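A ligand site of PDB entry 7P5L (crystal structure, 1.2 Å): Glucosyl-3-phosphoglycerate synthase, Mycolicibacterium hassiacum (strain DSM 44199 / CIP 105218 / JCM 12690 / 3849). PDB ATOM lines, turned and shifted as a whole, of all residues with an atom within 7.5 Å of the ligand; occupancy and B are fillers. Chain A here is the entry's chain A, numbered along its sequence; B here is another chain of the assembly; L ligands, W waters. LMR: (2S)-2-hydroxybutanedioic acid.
Water W1 lies within hydrogen-bond range of N of Arg 179 (3.0 Å) and O1A of the ligand (3.1 Å).
Water W2 lies within hydrogen-bond range of N of Gly 178 (3.0 Å), O2 of the ligand (3.2 Å) and NH2 of Arg 164 (3.4 Å).
Residues that only touch the ligand: Arg 255 (3.1 Å), Leu 260 (3.8 Å) and Met 263 (3.4 Å).
Hydrophobic or aromatic side chains within 4 Å of the ligand: Val 180, Leu 260 and Met 263.
Of the 27 residues printed, 8 come within 4 Å of the ligand.
The backbone NH of Thr 181 is in hydrogen-bond range of an oxygen (O1B) of the ligand (2.8 Å).
The side-chain hydroxyl (OG1) of Thr 181 is in hydrogen-bond range of an oxygen (O1B) of the ligand (2.8 Å).
The backbone NH of Val 180 is in hydrogen-bond range of an oxygen (O1A) of the ligand.
The backbone NH of Gly 178 sits close to an oxygen (O1B) of the ligand.
N of Arg 179 is in hydrogen-bond range of O1A of the ligand (3.3 Å).
The guanidinium group of Arg 253 is in salt-bridge range of an oxygen (O4B) of the ligand (3.3 Å).
O of Val 180 is in hydrogen-bond range of N of Ala 185 (2.9 Å).
The side-chain carboxylate (OD2) of Asp 133 is in salt-bridge range of the guanidinium group (NH1) of Arg 253 (3.2 Å).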
ATOM      1  N   LYS A 111      -5.702 -21.372   7.544  1.00  0.00           N
ATOM      2  CA  LYS A 111      -4.977 -20.715   8.618  1.00  0.00           C
ATOM      3  C   LYS A 111      -3.602 -21.343   8.834  1.00  0.00           C
ATOM      4  O   LYS A 111      -2.612 -20.638   9.019  1.00  0.00           O
ATOM      5  CB  LYS A 111      -5.789 -20.789   9.920  1.00  0.00           C
ATOM      6  CG  LYS A 111      -5.062 -20.160  11.103  1.00  0.00           C
ATOM      7  CD  LYS A 111      -5.686 -20.456  12.439  1.00  0.00           C
ATOM      8  CE  LYS A 111      -6.882 -19.603  12.694  1.00  0.00           C
ATOM      9  NZ  LYS A 111      -7.499 -19.816  14.020  1.00  0.00           N
ATOM     10  N   ASP A 131      -5.842 -14.583  17.278  1.00  0.00           N
ATOM     11  CA  ASP A 131      -6.798 -14.475  16.185  1.00  0.00           C
ATOM     12  C   ASP A 131      -7.196 -13.017  15.938  1.00  0.00           C
ATOM     13  O   ASP A 131      -7.320 -12.199  16.841  1.00  0.00           O
ATOM     14  CB  ASP A 131      -8.054 -15.322  16.474  1.00  0.00           C
ATOM     15  CG  ASP A 131      -7.869 -16.789  16.155  1.00  0.00           C
ATOM     16  OD1 ASP A 131      -7.025 -17.142  15.310  1.00  0.00           O
ATOM     17  OD2 ASP A 131      -8.594 -17.623  16.733  1.00  0.00           O
ATOM     18  N   ASP A 133     -10.092 -12.075  14.533  1.00  0.00           N
ATOM     19  CA  ASP A 133     -11.545 -11.952  14.559  1.00  0.00           C
ATOM     20  C   ASP A 133     -12.079 -11.732  15.961  1.00  0.00           C
ATOM     21  O   ASP A 133     -13.286 -11.777  16.161  1.00  0.00           O
ATOM     22  CB  ASP A 133     -12.235 -13.175  13.921  1.00  0.00           C
ATOM     23  CG  ASP A 133     -11.927 -14.491  14.618  1.00  0.00           C
ATOM     24  OD1 ASP A 133     -11.134 -14.488  15.564  1.00  0.00           O
ATOM     25  OD2 ASP A 133     -12.496 -15.536  14.209  1.00  0.00           O
ATOM     26  N   ARG A 164     -15.969 -18.814  30.857  1.00  0.00           N
ATOM     27  CA  ARG A 164     -17.191 -18.515  30.122  1.00  0.00           C
ATOM     28  C   ARG A 164     -18.206 -17.844  31.036  1.00  0.00           C
ATOM     29  O   ARG A 164     -18.244 -18.114  32.239  1.00  0.00           O
ATOM     30  CB  ARG A 164     -17.785 -19.814  29.568  1.00  0.00           C
ATOM     31  CG  ARG A 164     -16.819 -20.609  28.697  1.00  0.00           C
ATOM     32  CD  ARG A 164     -16.345 -19.773  27.520  1.00  0.00           C
ATOM     33  NE  ARG A 164     -15.508 -20.529  26.588  1.00  0.00           N
ATOM     34  CZ  ARG A 164     -14.947 -20.015  25.502  1.00  0.00           C
ATOM     35  NH1 ARG A 164     -15.099 -18.737  25.191  1.00  0.00           N
ATOM     36  NH2 ARG A 164     -14.203 -20.794  24.718  1.00  0.00           N
ATOM     37  N   GLY A 176     -14.848 -23.898  29.668  1.00  0.00           N
ATOM     38  CA  GLY A 176     -14.481 -24.859  28.655  1.00  0.00           C
ATOM     39  C   GLY A 176     -14.888 -24.443  27.240  1.00  0.00           C
ATOM     40  O   GLY A 176     -15.254 -23.291  27.015  1.00  0.00           O
ATOM     41  N   GLY A 177     -14.856 -25.397  26.304  1.00  0.00           N
ATOM     42  CA  GLY A 177     -14.903 -25.080  24.887  1.00  0.00           C
ATOM     43  C   GLY A 177     -16.300 -25.183  24.272  1.00  0.00           C
ATOM     44  O   GLY A 177     -17.290 -25.494  24.927  1.00  0.00           O
ATOM     45  N   GLY A 178     -16.342 -24.894  22.974  1.00  0.00           N
ATOM     46  CA  GLY A 178     -17.561 -25.015  22.198  1.00  0.00           C
ATOM     47  C   GLY A 178     -17.828 -26.447  21.776  1.00  0.00           C
ATOM     48  O   GLY A 178     -17.249 -27.403  22.297  1.00  0.00           O
ATOM     49  N   ARG A 179     -18.713 -26.585  20.798  1.00  0.00           N
ATOM     50  CA  ARG A 179     -19.195 -27.917  20.444  1.00  0.00           C
ATOM     51  C   ARG A 179     -18.116 -28.763  19.770  1.00  0.00           C
ATOM     52  O   ARG A 179     -18.060 -29.965  19.998  1.00  0.00           O
ATOM     53  CB  ARG A 179     -20.439 -27.811  19.572  1.00  0.00           C
ATOM     54  CG  ARG A 179     -21.746 -27.595  20.364  1.00  0.00           C
ATOM     55  CD  ARG A 179     -21.559 -26.911  21.713  1.00  0.00           C
ATOM     56  NE  ARG A 179     -22.827 -26.494  22.290  1.00  0.00           N
ATOM     57  CZ  ARG A 179     -22.946 -25.848  23.446  1.00  0.00           C
ATOM     58  NH1 ARG A 179     -21.887 -25.509  24.161  1.00  0.00           N
ATOM     59  NH2 ARG A 179     -24.163 -25.528  23.896  1.00  0.00           N
ATOM     60  N   VAL A 180     -17.279 -28.178  18.908  1.00  0.00           N
ATOM     61  CA  VAL A 180     -16.219 -28.981  18.326  1.00  0.00           C
ATOM     62  C   VAL A 180     -15.229 -29.397  19.399  1.00  0.00           C
ATOM     63  O   VAL A 180     -14.765 -30.539  19.432  1.00  0.00           O
ATOM     64  CB  VAL A 180     -15.546 -28.277  17.142  1.00  0.00           C
ATOM     65  CG1 VAL A 180     -14.460 -29.164  16.534  1.00  0.00           C
ATOM     66  CG2 VAL A 180     -16.577 -27.900  16.103  1.00  0.00           C
ATOM     67  N   THR A 181     -14.921 -28.489  20.314  1.00  0.00           N
ATOM     68  CA  THR A 181     -14.001 -28.832  21.390  1.00  0.00           C
ATOM     69  C   THR A 181     -14.547 -29.959  22.252  1.00  0.00           C
ATOM     70  O   THR A 181     -13.831 -30.900  22.572  1.00  0.00           O
ATOM     71  CB  THR A 181     -13.732 -27.604  22.255  1.00  0.00           C
ATOM     72  OG1 THR A 181     -13.031 -26.618  21.477  1.00  0.00           O
ATOM     73  CG2 THR A 181     -12.882 -27.952  23.448  1.00  0.00           C
ATOM     74  N   GLU A 182     -15.806 -29.851  22.669  1.00  0.00           N
ATOM     75  CA  GLU A 182     -16.321 -30.784  23.665  1.00  0.00           C
ATOM     76  C   GLU A 182     -16.823 -32.075  23.053  1.00  0.00           C
ATOM     77  O   GLU A 182     -16.842 -33.093  23.734  1.00  0.00           O
ATOM     78  CB  GLU A 182     -17.416 -30.139  24.509  1.00  0.00           C
ATOM     79  CG  GLU A 182     -16.925 -28.954  25.324  1.00  0.00           C
ATOM     80  CD  GLU A 182     -15.716 -29.231  26.230  1.00  0.00           C
ATOM     81  OE1 GLU A 182     -15.448 -30.373  26.651  1.00  0.00           O
ATOM     82  OE2 GLU A 182     -15.032 -28.243  26.557  1.00  0.00           O
ATOM     83  N   LEU A 183     -17.276 -32.056  21.797  1.00  0.00           N
ATOM     84  CA  LEU A 183     -17.780 -33.264  21.176  1.00  0.00           C
ATOM     85  C   LEU A 183     -16.748 -33.985  20.324  1.00  0.00           C
ATOM     86  O   LEU A 183     -16.872 -35.193  20.113  1.00  0.00           O
ATOM     87  CB  LEU A 183     -18.998 -32.961  20.297  1.00  0.00           C
ATOM     88  CG  LEU A 183     -20.174 -32.317  21.032  1.00  0.00           C
ATOM     89  CD1 LEU A 183     -21.365 -32.145  20.097  1.00  0.00           C
ATOM     90  CD2 LEU A 183     -20.557 -33.089  22.304  1.00  0.00           C
ATOM     91  N   ALA A 185     -12.828 -32.722  19.714  1.00  0.00           N
ATOM     92  CA  ALA A 185     -11.421 -32.703  20.099  1.00  0.00           C
ATOM     93  C   ALA A 185     -11.178 -33.414  21.421  1.00  0.00           C
ATOM     94  O   ALA A 185     -10.290 -34.269  21.504  1.00  0.00           O
ATOM     95  CB  ALA A 185     -10.912 -31.270  20.154  1.00  0.00           C
ATOM     96  N   GLN A 201      -8.846 -25.817  26.369  1.00  0.00           N
ATOM     97  CA  GLN A 201      -9.294 -25.322  25.067  1.00  0.00           C
ATOM     98  C   GLN A 201      -8.246 -25.642  24.012  1.00  0.00           C
ATOM     99  O   GLN A 201      -7.507 -24.755  23.551  1.00  0.00           O
ATOM    100  CB  GLN A 201      -9.677 -23.845  25.149  1.00  0.00           C
ATOM    101  CG  GLN A 201     -11.046 -23.681  25.843  1.00  0.00           C
ATOM    102  CD  GLN A 201     -11.297 -22.321  26.408  1.00  0.00           C
ATOM    103  OE1 GLN A 201     -10.793 -21.308  25.919  1.00  0.00           O
ATOM    104  NE2 GLN A 201     -12.076 -22.281  27.462  1.00  0.00           N
ATOM    105  N   LEU A 203      -8.321 -26.223  20.906  1.00  0.00           N
ATOM    106  CA  LEU A 203      -8.497 -25.610  19.599  1.00  0.00           C
ATOM    107  C   LEU A 203      -8.310 -24.101  19.625  1.00  0.00           C
ATOM    108  O   LEU A 203      -8.464 -23.448  18.586  1.00  0.00           O
ATOM    109  CB  LEU A 203      -9.890 -25.942  19.022  1.00  0.00           C
ATOM    110  CG  LEU A 203     -10.244 -27.444  18.978  1.00  0.00           C
ATOM    111  CD1 LEU A 203     -11.582 -27.623  18.299  1.00  0.00           C
ATOM    112  CD2 LEU A 203      -9.163 -28.248  18.289  1.00  0.00           C
ATOM    113  N   GLY A 204      -7.971 -23.533  20.772  1.00  0.00           N
ATOM    114  CA  GLY A 204      -7.893 -22.080  20.894  1.00  0.00           C
ATOM    115  C   GLY A 204      -6.845 -21.473  19.962  1.00  0.00           C
ATOM    116  O   GLY A 204      -5.783 -22.038  19.733  1.00  0.00           O
ATOM    117  N   GLY A 205      -7.154 -20.272  19.465  1.00  0.00           N
ATOM    118  CA  GLY A 205      -6.276 -19.556  18.572  1.00  0.00           C
ATOM    119  C   GLY A 205      -5.271 -18.640  19.216  1.00  0.00           C
ATOM    120  O   GLY A 205      -4.458 -18.032  18.516  1.00  0.00           O
ATOM    121  N   TYR A 223      -8.081 -25.699   9.623  1.00  0.00           N
ATOM    122  CA  TYR A 223      -8.605 -25.786  10.979  1.00  0.00           C
ATOM    123  C   TYR A 223      -7.884 -26.833  11.829  1.00  0.00           C
ATOM    124  O   TYR A 223      -8.250 -26.995  12.989  1.00  0.00           O
ATOM    125  CB  TYR A 223     -10.093 -26.180  10.917  1.00  0.00           C
ATOM    126  CG  TYR A 223     -11.054 -25.144  10.432  1.00  0.00           C
ATOM    127  CD1 TYR A 223     -11.085 -23.898  11.008  1.00  0.00           C
ATOM    128  CD2 TYR A 223     -11.958 -25.431   9.415  1.00  0.00           C
ATOM    129  CE1 TYR A 223     -11.984 -22.938  10.592  1.00  0.00           C
ATOM    130  CE2 TYR A 223     -12.876 -24.483   9.001  1.00  0.00           C
ATOM    131  CZ  TYR A 223     -12.874 -23.244   9.581  1.00  0.00           C
ATOM    132  OH  TYR A 223     -13.770 -22.296   9.173  1.00  0.00           O
ATOM    133  N   GLU A 226      -4.091 -25.849  15.177  1.00  0.00           N
ATOM    134  CA  GLU A 226      -3.906 -25.742  16.628  1.00  0.00           C
ATOM    135  C   GLU A 226      -3.753 -27.106  17.287  1.00  0.00           C
ATOM    136  O   GLU A 226      -2.870 -27.303  18.135  1.00  0.00           O
ATOM    137  CB  GLU A 226      -5.043 -24.948  17.285  1.00  0.00           C
ATOM    138  CG  GLU A 226      -5.235 -23.542  16.723  1.00  0.00           C
ATOM    139  CD  GLU A 226      -6.229 -23.441  15.584  1.00  0.00           C
ATOM    140  OE1 GLU A 226      -6.728 -24.471  15.061  1.00  0.00           O
ATOM    141  OE2 GLU A 226      -6.486 -22.289  15.173  1.00  0.00           O
ATOM    142  N   HIS A 252     -18.944 -17.807  24.249  1.00  0.00           N
ATOM    143  CA  HIS A 252     -18.703 -18.668  23.110  1.00  0.00           C
ATOM    144  C   HIS A 252     -19.094 -17.955  21.818  1.00  0.00           C
ATOM    145  O   HIS A 252     -20.122 -17.277  21.747  1.00  0.00           O
ATOM    146  CB  HIS A 252     -19.526 -19.955  23.231  1.00  0.00           C
ATOM    147  CG  HIS A 252     -19.074 -20.864  24.328  1.00  0.00           C
ATOM    148  ND1 HIS A 252     -17.931 -21.628  24.241  1.00  0.00           N
ATOM    149  CD2 HIS A 252     -19.613 -21.122  25.540  1.00  0.00           C
ATOM    150  CE1 HIS A 252     -17.780 -22.314  25.357  1.00  0.00           C
ATOM    151  NE2 HIS A 252     -18.796 -22.032  26.164  1.00  0.00           N
ATOM    152  N   ARG A 253     -18.255 -18.107  20.797  1.00  0.00           N
ATOM    153  CA  ARG A 253     -18.656 -17.732  19.448  1.00  0.00           C
ATOM    154  C   ARG A 253     -19.696 -18.727  18.953  1.00  0.00           C
ATOM    155  O   ARG A 253     -19.688 -19.906  19.327  1.00  0.00           O
ATOM    156  CB  ARG A 253     -17.451 -17.741  18.510  1.00  0.00           C
ATOM    157  CG  ARG A 253     -17.523 -16.720  17.384  1.00  0.00           C
ATOM    158  CD  ARG A 253     -16.457 -16.973  16.304  1.00  0.00           C
ATOM    159  NE  ARG A 253     -15.338 -17.799  16.778  1.00  0.00           N
ATOM    160  CZ  ARG A 253     -14.136 -17.345  17.122  1.00  0.00           C
ATOM    161  NH1 ARG A 253     -13.844 -16.056  17.065  1.00  0.00           N
ATOM    162  NH2 ARG A 253     -13.211 -18.198  17.527  1.00  0.00           N
ATOM    163  N   ASN A 254     -20.601 -18.257  18.108  1.00  0.00           N
ATOM    164  CA  ASN A 254     -21.645 -19.105  17.522  1.00  0.00           C
ATOM    165  C   ASN A 254     -21.443 -19.125  16.008  1.00  0.00           C
ATOM    166  O   ASN A 254     -21.974 -18.264  15.289  1.00  0.00           O
ATOM    167  CB  ASN A 254     -23.042 -18.659  17.913  1.00  0.00           C
ATOM    168  CG  ASN A 254     -24.129 -19.564  17.337  1.00  0.00           C
ATOM    169  OD1 ASN A 254     -24.994 -19.116  16.584  1.00  0.00           O
ATOM    170  ND2 ASN A 254     -24.062 -20.845  17.685  1.00  0.00           N
ATOM    171  N   ARG A 255     -20.667 -20.106  15.549  1.00  0.00           N
ATOM    172  CA  ARG A 255     -20.363 -20.261  14.108  1.00  0.00           C
ATOM    173  C   ARG A 255     -21.462 -21.129  13.489  1.00  0.00           C
ATOM    174  O   ARG A 255     -22.061 -21.943  14.210  1.00  0.00           O
ATOM    175  CB  ARG A 255     -18.970 -20.890  13.908  1.00  0.00           C
ATOM    176  CG  ARG A 255     -17.806 -20.031  14.431  1.00  0.00           C
ATOM    177  CD  ARG A 255     -16.406 -20.606  14.083  1.00  0.00           C
ATOM    178  N   ASP A 259     -19.713 -24.621   9.071  1.00  0.00           N
ATOM    179  CA  ASP A 259     -18.329 -24.321   9.408  1.00  0.00           C
ATOM    180  C   ASP A 259     -17.823 -25.218  10.527  1.00  0.00           C
ATOM    181  O   ASP A 259     -16.677 -25.685  10.492  1.00  0.00           O
ATOM    182  CB  ASP A 259     -18.186 -22.861   9.837  1.00  0.00           C
ATOM    183  CG  ASP A 259     -18.126 -21.892   8.668  1.00  0.00           C
ATOM    184  OD1 ASP A 259     -17.961 -22.340   7.511  1.00  0.00           O
ATOM    185  OD2 ASP A 259     -18.243 -20.672   8.918  1.00  0.00           O
ATOM    186  N   LEU A 260     -18.655 -25.453  11.553  1.00  0.00           N
ATOM    187  CA  LEU A 260     -18.248 -26.372  12.617  1.00  0.00           C
ATOM    188  C   LEU A 260     -18.007 -27.769  12.090  1.00  0.00           C
ATOM    189  O   LEU A 260     -17.085 -28.447  12.542  1.00  0.00           O
ATOM    190  CB  LEU A 260     -19.297 -26.405  13.714  1.00  0.00           C
ATOM    191  CG  LEU A 260     -19.540 -25.076  14.416  1.00  0.00           C
ATOM    192  CD1 LEU A 260     -20.701 -25.220  15.375  1.00  0.00           C
ATOM    193  CD2 LEU A 260     -18.283 -24.596  15.133  1.00  0.00           C
ATOM    194  N   MET A 263     -14.668 -27.758  10.395  1.00  0.00           N
ATOM    195  CA  MET A 263     -13.654 -27.750  11.432  1.00  0.00           C
ATOM    196  C   MET A 263     -13.489 -29.143  12.023  1.00  0.00           C
ATOM    197  O   MET A 263     -12.367 -29.633  12.184  1.00  0.00           O
ATOM    198  CB  MET A 263     -14.044 -26.752  12.517  1.00  0.00           C
ATOM    199  CG  MET A 263     -13.015 -26.619  13.610  1.00  0.00           C
ATOM    200  SD  MET A 263     -13.606 -25.593  14.965  1.00  0.00           S
ATOM    201  CE  MET A 263     -14.066 -24.066  14.133  1.00  0.00           C
ATOM    202  N   LEU B 183     -21.227 -33.457  13.788  1.00  0.00           N
ATOM    203  CA  LEU B 183     -19.846 -33.136  14.118  1.00  0.00           C
ATOM    204  C   LEU B 183     -19.026 -34.379  14.416  1.00  0.00           C
ATOM    205  O   LEU B 183     -17.794 -34.316  14.307  1.00  0.00           O
ATOM    206  CB  LEU B 183     -19.781 -32.184  15.313  1.00  0.00           C
ATOM    207  CG  LEU B 183     -20.533 -30.858  15.168  1.00  0.00           C
ATOM    208  CD1 LEU B 183     -20.280 -29.984  16.387  1.00  0.00           C
ATOM    209  CD2 LEU B 183     -20.156 -30.127  13.892  1.00  0.00           C
HETATM  210  C1  LMR L   1     -15.716 -25.058  19.153  1.00  0.00           C
HETATM  211  O1A LMR L   1     -16.714 -25.382  18.499  1.00  0.00           O
HETATM  212  O1B LMR L   1     -15.233 -25.714  20.085  1.00  0.00           O
HETATM  213  C2  LMR L   1     -15.066 -23.718  18.796  1.00  0.00           C
HETATM  214  O2  LMR L   1     -13.727 -23.634  19.244  1.00  0.00           O
HETATM  215  C3  LMR L   1     -15.134 -23.448  17.283  1.00  0.00           C
HETATM  216  C4  LMR L   1     -14.620 -22.062  16.939  1.00  0.00           C
HETATM  217  O4A LMR L   1     -13.417 -21.933  16.659  1.00  0.00           O
HETATM  218  O4B LMR L   1     -15.422 -21.111  16.946  1.00  0.00           O
HETATM  219  O   HOH W   1     -19.532 -24.312  19.105  1.00  0.00           O
HETATM  220  O   HOH W   2     -13.894 -23.212  22.374  1.00  0.00           O
